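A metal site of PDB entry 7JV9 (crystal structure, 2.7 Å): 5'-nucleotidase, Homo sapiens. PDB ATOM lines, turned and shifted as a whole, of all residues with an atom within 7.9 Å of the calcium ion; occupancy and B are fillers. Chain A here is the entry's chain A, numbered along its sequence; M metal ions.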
ATOM      1  N   LYS A 184     -19.133  22.934   6.196  1.00  0.00           N
ATOM      2  CA  LYS A 184     -18.326  22.159   7.162  1.00  0.00           C
ATOM      3  C   LYS A 184     -17.721  23.057   8.246  1.00  0.00           C
ATOM      4  O   LYS A 184     -17.761  22.718   9.423  1.00  0.00           O
ATOM      5  CB  LYS A 184     -17.225  21.337   6.479  1.00  0.00           C
ATOM      6  CG  LYS A 184     -17.746  20.217   5.581  1.00  0.00           C
ATOM      7  CD  LYS A 184     -18.649  19.247   6.324  1.00  0.00           C
ATOM      8  CE  LYS A 184     -18.809  17.949   5.569  1.00  0.00           C
ATOM      9  NZ  LYS A 184     -19.662  17.015   6.348  1.00  0.00           N
ATOM     10  N   VAL A 188     -21.698  22.084  10.128  1.00  0.00           N
ATOM     11  CA  VAL A 188     -22.832  21.403   9.496  1.00  0.00           C
ATOM     12  C   VAL A 188     -22.312  20.080   8.928  1.00  0.00           C
ATOM     13  O   VAL A 188     -21.681  20.050   7.855  1.00  0.00           O
ATOM     14  CB  VAL A 188     -23.499  22.250   8.385  1.00  0.00           C
ATOM     15  CG1 VAL A 188     -24.681  21.522   7.780  1.00  0.00           C
ATOM     16  CG2 VAL A 188     -24.001  23.547   8.961  1.00  0.00           C
ATOM     17  N   ASN A 189     -22.568  19.005   9.666  1.00  0.00           N
ATOM     18  CA  ASN A 189     -21.988  17.683   9.362  1.00  0.00           C
ATOM     19  C   ASN A 189     -22.826  16.789   8.428  1.00  0.00           C
ATOM     20  O   ASN A 189     -22.328  15.794   7.899  1.00  0.00           O
ATOM     21  CB  ASN A 189     -21.620  16.942  10.661  1.00  0.00           C
ATOM     22  CG  ASN A 189     -22.819  16.655  11.571  1.00  0.00           C
ATOM     23  OD1 ASN A 189     -23.946  16.483  11.108  1.00  0.00           O
ATOM     24  ND2 ASN A 189     -22.568  16.577  12.870  1.00  0.00           N
ATOM     25  N   LYS A 190     -24.096  17.166   8.221  1.00  0.00           N
ATOM     26  CA  LYS A 190     -25.023  16.442   7.325  1.00  0.00           C
ATOM     27  C   LYS A 190     -25.388  17.305   6.139  1.00  0.00           C
ATOM     28  O   LYS A 190     -26.005  18.357   6.310  1.00  0.00           O
ATOM     29  CB  LYS A 190     -26.287  16.016   8.067  1.00  0.00           C
ATOM     30  CG  LYS A 190     -26.059  14.884   9.073  1.00  0.00           C
ATOM     31  CD  LYS A 190     -27.226  14.752  10.023  1.00  0.00           C
ATOM     32  CE  LYS A 190     -27.216  15.798  11.126  1.00  0.00           C
ATOM     33  NZ  LYS A 190     -26.465  15.292  12.299  1.00  0.00           N
ATOM     34  N   ILE A 191     -25.025  16.852   4.942  1.00  0.00           N
ATOM     35  CA  ILE A 191     -25.135  17.679   3.738  1.00  0.00           C
ATOM     36  C   ILE A 191     -25.837  16.930   2.592  1.00  0.00           C
ATOM     37  O   ILE A 191     -25.384  15.877   2.151  1.00  0.00           O
ATOM     38  CB  ILE A 191     -23.764  18.259   3.328  1.00  0.00           C
ATOM     39  CG1 ILE A 191     -23.349  19.318   4.362  1.00  0.00           C
ATOM     40  CG2 ILE A 191     -23.825  18.886   1.923  1.00  0.00           C
ATOM     41  CD1 ILE A 191     -22.026  20.005   4.151  1.00  0.00           C
ATOM     42  N   ILE A 192     -26.934  17.518   2.138  1.00  0.00           N
ATOM     43  CA  ILE A 192     -27.727  17.031   1.022  1.00  0.00           C
ATOM     44  C   ILE A 192     -27.519  17.952  -0.165  1.00  0.00           C
ATOM     45  O   ILE A 192     -27.613  19.168  -0.034  1.00  0.00           O
ATOM     46  CB  ILE A 192     -29.233  17.044   1.360  1.00  0.00           C
ATOM     47  CG1 ILE A 192     -29.513  16.198   2.611  1.00  0.00           C
ATOM     48  CG2 ILE A 192     -30.059  16.549   0.171  1.00  0.00           C
ATOM     49  CD1 ILE A 192     -30.930  16.311   3.135  1.00  0.00           C
ATOM     50  N   GLY A 211     -17.607  15.912   1.042  1.00  0.00           N
ATOM     51  CA  GLY A 211     -18.553  16.374   2.081  1.00  0.00           C
ATOM     52  C   GLY A 211     -20.029  16.044   1.884  1.00  0.00           C
ATOM     53  O   GLY A 211     -20.793  16.045   2.857  1.00  0.00           O
ATOM     54  N   VAL A 212     -20.437  15.799   0.621  1.00  0.00           N
ATOM     55  CA  VAL A 212     -21.836  15.497   0.279  1.00  0.00           C
ATOM     56  C   VAL A 212     -22.224  14.098   0.747  1.00  0.00           C
ATOM     57  O   VAL A 212     -21.542  13.123   0.429  1.00  0.00           O
ATOM     58  CB  VAL A 212     -22.083  15.575  -1.238  1.00  0.00           C
ATOM     59  CG1 VAL A 212     -23.444  14.992  -1.596  1.00  0.00           C
ATOM     60  CG2 VAL A 212     -22.035  17.021  -1.700  1.00  0.00           C
ATOM     61  N   ASP A 213     -23.316  14.005   1.489  1.00  0.00           N
ATOM     62  CA  ASP A 213     -23.746  12.751   2.079  1.00  0.00           C
ATOM     63  C   ASP A 213     -24.828  12.064   1.249  1.00  0.00           C
ATOM     64  O   ASP A 213     -24.967  10.855   1.329  1.00  0.00           O
ATOM     65  CB  ASP A 213     -24.237  12.969   3.514  1.00  0.00           C
ATOM     66  CG  ASP A 213     -23.140  13.479   4.449  1.00  0.00           C
ATOM     67  OD1 ASP A 213     -22.018  12.920   4.523  1.00  0.00           O
ATOM     68  OD2 ASP A 213     -23.409  14.476   5.160  1.00  0.00           O
ATOM     69  N   VAL A 214     -25.602  12.835   0.492  1.00  0.00           N
ATOM     70  CA  VAL A 214     -26.757  12.349  -0.287  1.00  0.00           C
ATOM     71  C   VAL A 214     -26.975  13.278  -1.474  1.00  0.00           C
ATOM     72  O   VAL A 214     -26.860  14.490  -1.331  1.00  0.00           O
ATOM     73  CB  VAL A 214     -28.094  12.409   0.502  1.00  0.00           C
ATOM     74  CG1 VAL A 214     -29.192  11.688  -0.259  1.00  0.00           C
ATOM     75  CG2 VAL A 214     -27.981  11.830   1.901  1.00  0.00           C
ATOM     76  N   ARG A 249     -16.257   6.930   0.540  1.00  0.00           N
ATOM     77  CA  ARG A 249     -17.587   6.824   1.177  1.00  0.00           C
ATOM     78  C   ARG A 249     -18.694   6.383   0.227  1.00  0.00           C
ATOM     79  O   ARG A 249     -18.647   6.657  -0.977  1.00  0.00           O
ATOM     80  CB  ARG A 249     -17.981   8.144   1.807  1.00  0.00           C
ATOM     81  CG  ARG A 249     -17.063   8.589   2.937  1.00  0.00           C
ATOM     82  CD  ARG A 249     -17.516   9.908   3.540  1.00  0.00           C
ATOM     83  NE  ARG A 249     -17.498  10.945   2.513  1.00  0.00           N
ATOM     84  CZ  ARG A 249     -18.551  11.555   1.984  1.00  0.00           C
ATOM     85  NH1 ARG A 249     -19.797  11.302   2.375  1.00  0.00           N
ATOM     86  NH2 ARG A 249     -18.349  12.483   1.034  1.00  0.00           N
ATOM     87  N   PHE A 270     -27.821   8.170  10.179  1.00  0.00           N
ATOM     88  CA  PHE A 270     -26.594   8.942  10.376  1.00  0.00           C
ATOM     89  C   PHE A 270     -25.969   8.626  11.729  1.00  0.00           C
ATOM     90  O   PHE A 270     -26.686   8.295  12.669  1.00  0.00           O
ATOM     91  CB  PHE A 270     -26.905  10.432  10.361  1.00  0.00           C
ATOM     92  CG  PHE A 270     -27.025  11.041   9.003  1.00  0.00           C
ATOM     93  CD1 PHE A 270     -25.906  11.212   8.196  1.00  0.00           C
ATOM     94  CD2 PHE A 270     -28.258  11.499   8.542  1.00  0.00           C
ATOM     95  CE1 PHE A 270     -26.015  11.799   6.930  1.00  0.00           C
ATOM     96  CE2 PHE A 270     -28.375  12.093   7.277  1.00  0.00           C
ATOM     97  CZ  PHE A 270     -27.244  12.244   6.479  1.00  0.00           C
ATOM     98  N   ASP A 271     -24.655   8.767  11.817  1.00  0.00           N
ATOM     99  CA  ASP A 271     -23.979   8.804  13.136  1.00  0.00           C
ATOM    100  C   ASP A 271     -23.925  10.255  13.675  1.00  0.00           C
ATOM    101  O   ASP A 271     -24.344  11.199  13.001  1.00  0.00           O
ATOM    102  CB  ASP A 271     -22.579   8.142  13.109  1.00  0.00           C
ATOM    103  CG  ASP A 271     -21.563   8.867  12.226  1.00  0.00           C
ATOM    104  OD1 ASP A 271     -21.807   9.994  11.762  1.00  0.00           O
ATOM    105  OD2 ASP A 271     -20.483   8.285  12.012  1.00  0.00           O
ATOM    106  N   ARG A 273     -21.564  12.253  13.847  1.00  0.00           N
ATOM    107  CA  ARG A 273     -20.697  13.115  13.039  1.00  0.00           C
ATOM    108  C   ARG A 273     -21.221  13.302  11.601  1.00  0.00           C
ATOM    109  O   ARG A 273     -20.481  13.730  10.699  1.00  0.00           O
ATOM    110  CB  ARG A 273     -19.286  12.526  13.024  1.00  0.00           C
ATOM    111  CG  ARG A 273     -18.703  12.278  14.412  1.00  0.00           C
ATOM    112  CD  ARG A 273     -17.229  11.907  14.331  1.00  0.00           C
ATOM    113  NE  ARG A 273     -16.403  13.004  13.823  1.00  0.00           N
ATOM    114  CZ  ARG A 273     -15.088  12.941  13.609  1.00  0.00           C
ATOM    115  NH1 ARG A 273     -14.401  11.822  13.860  1.00  0.00           N
ATOM    116  NH2 ARG A 273     -14.454  14.004  13.141  1.00  0.00           N
ATOM    117  N   GLY A 274     -22.485  12.951  11.364  1.00  0.00           N
ATOM    118  CA  GLY A 274     -23.117  13.170  10.063  1.00  0.00           C
ATOM    119  C   GLY A 274     -22.678  12.299   8.886  1.00  0.00           C
ATOM    120  O   GLY A 274     -22.867  12.662   7.711  1.00  0.00           O
ATOM    121  N   ASN A 275     -22.101  11.144   9.209  1.00  0.00           N
ATOM    122  CA  ASN A 275     -21.764  10.131   8.214  1.00  0.00           C
ATOM    123  C   ASN A 275     -22.918   9.160   8.026  1.00  0.00           C
ATOM    124  O   ASN A 275     -23.572   8.760   8.988  1.00  0.00           O
ATOM    125  CB  ASN A 275     -20.539   9.335   8.656  1.00  0.00           C
ATOM    126  CG  ASN A 275     -19.283  10.169   8.645  1.00  0.00           C
ATOM    127  OD1 ASN A 275     -18.926  10.717   7.609  1.00  0.00           O
ATOM    128  ND2 ASN A 275     -18.611  10.266   9.794  1.00  0.00           N
ATOM    129  N   VAL A 276     -23.127   8.774   6.769  1.00  0.00           N
ATOM    130  CA  VAL A 276     -24.174   7.842   6.417  1.00  0.00           C
ATOM    131  C   VAL A 276     -23.714   6.427   6.781  1.00  0.00           C
ATOM    132  O   VAL A 276     -22.777   5.891   6.196  1.00  0.00           O
ATOM    133  CB  VAL A 276     -24.556   7.957   4.929  1.00  0.00           C
ATOM    134  CG1 VAL A 276     -25.613   6.927   4.527  1.00  0.00           C
ATOM    135  CG2 VAL A 276     -25.109   9.353   4.651  1.00  0.00           C
HETATM  136 CA    CA M   1     -21.443  14.196   6.583  1.00  0.00          CA
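O of Asn 189 lies close to NZ of Lys 184, at 3.3 Å. The side-chain carboxylate (OD1) of Asp 213 lies close to the guanidinium group (NH1) of Arg 249 (3.5 Å). The backbone NH of Asp 213 lies within hydrogen-bond range of the backbone carbonyl oxygen of Ile 191, at 2.9 Å. The side-chain amide oxygen (OD1) of Asn 189 sits at hydrogen-bond distance from the side-chain amino group (NZ) of Lys 190 (3.0 Å). The backbone NH (N) of Gly 274 sits at hydrogen-bond distance from the side-chain carboxylate (OD1) of Asp 271.
Merely in contact with the calcium ion: Lys 184 (3.3 Å). Of the 17 residues printed, 4 come within 4 Å of the calcium ion. Along chain A the residues within 4 Å of the calcium ion span positions 184 to 274. The nearest printed residue that does not touch the calcium ion is Asn 275 (4.1 Å).
The calcium ion is bound by the backbone carbonyl oxygen (O) of Asn 189 (2.3 Å), the backbone carbonyl oxygen (O) of Gly 274 (2.4 Å), the side-chain carboxylate (OD2) of Asp 213 (2.4 Å) and the side-chain carboxylate (OD1) of Asp 213 (2.5 Å). The calcium ion has four donor atoms within binding distance.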
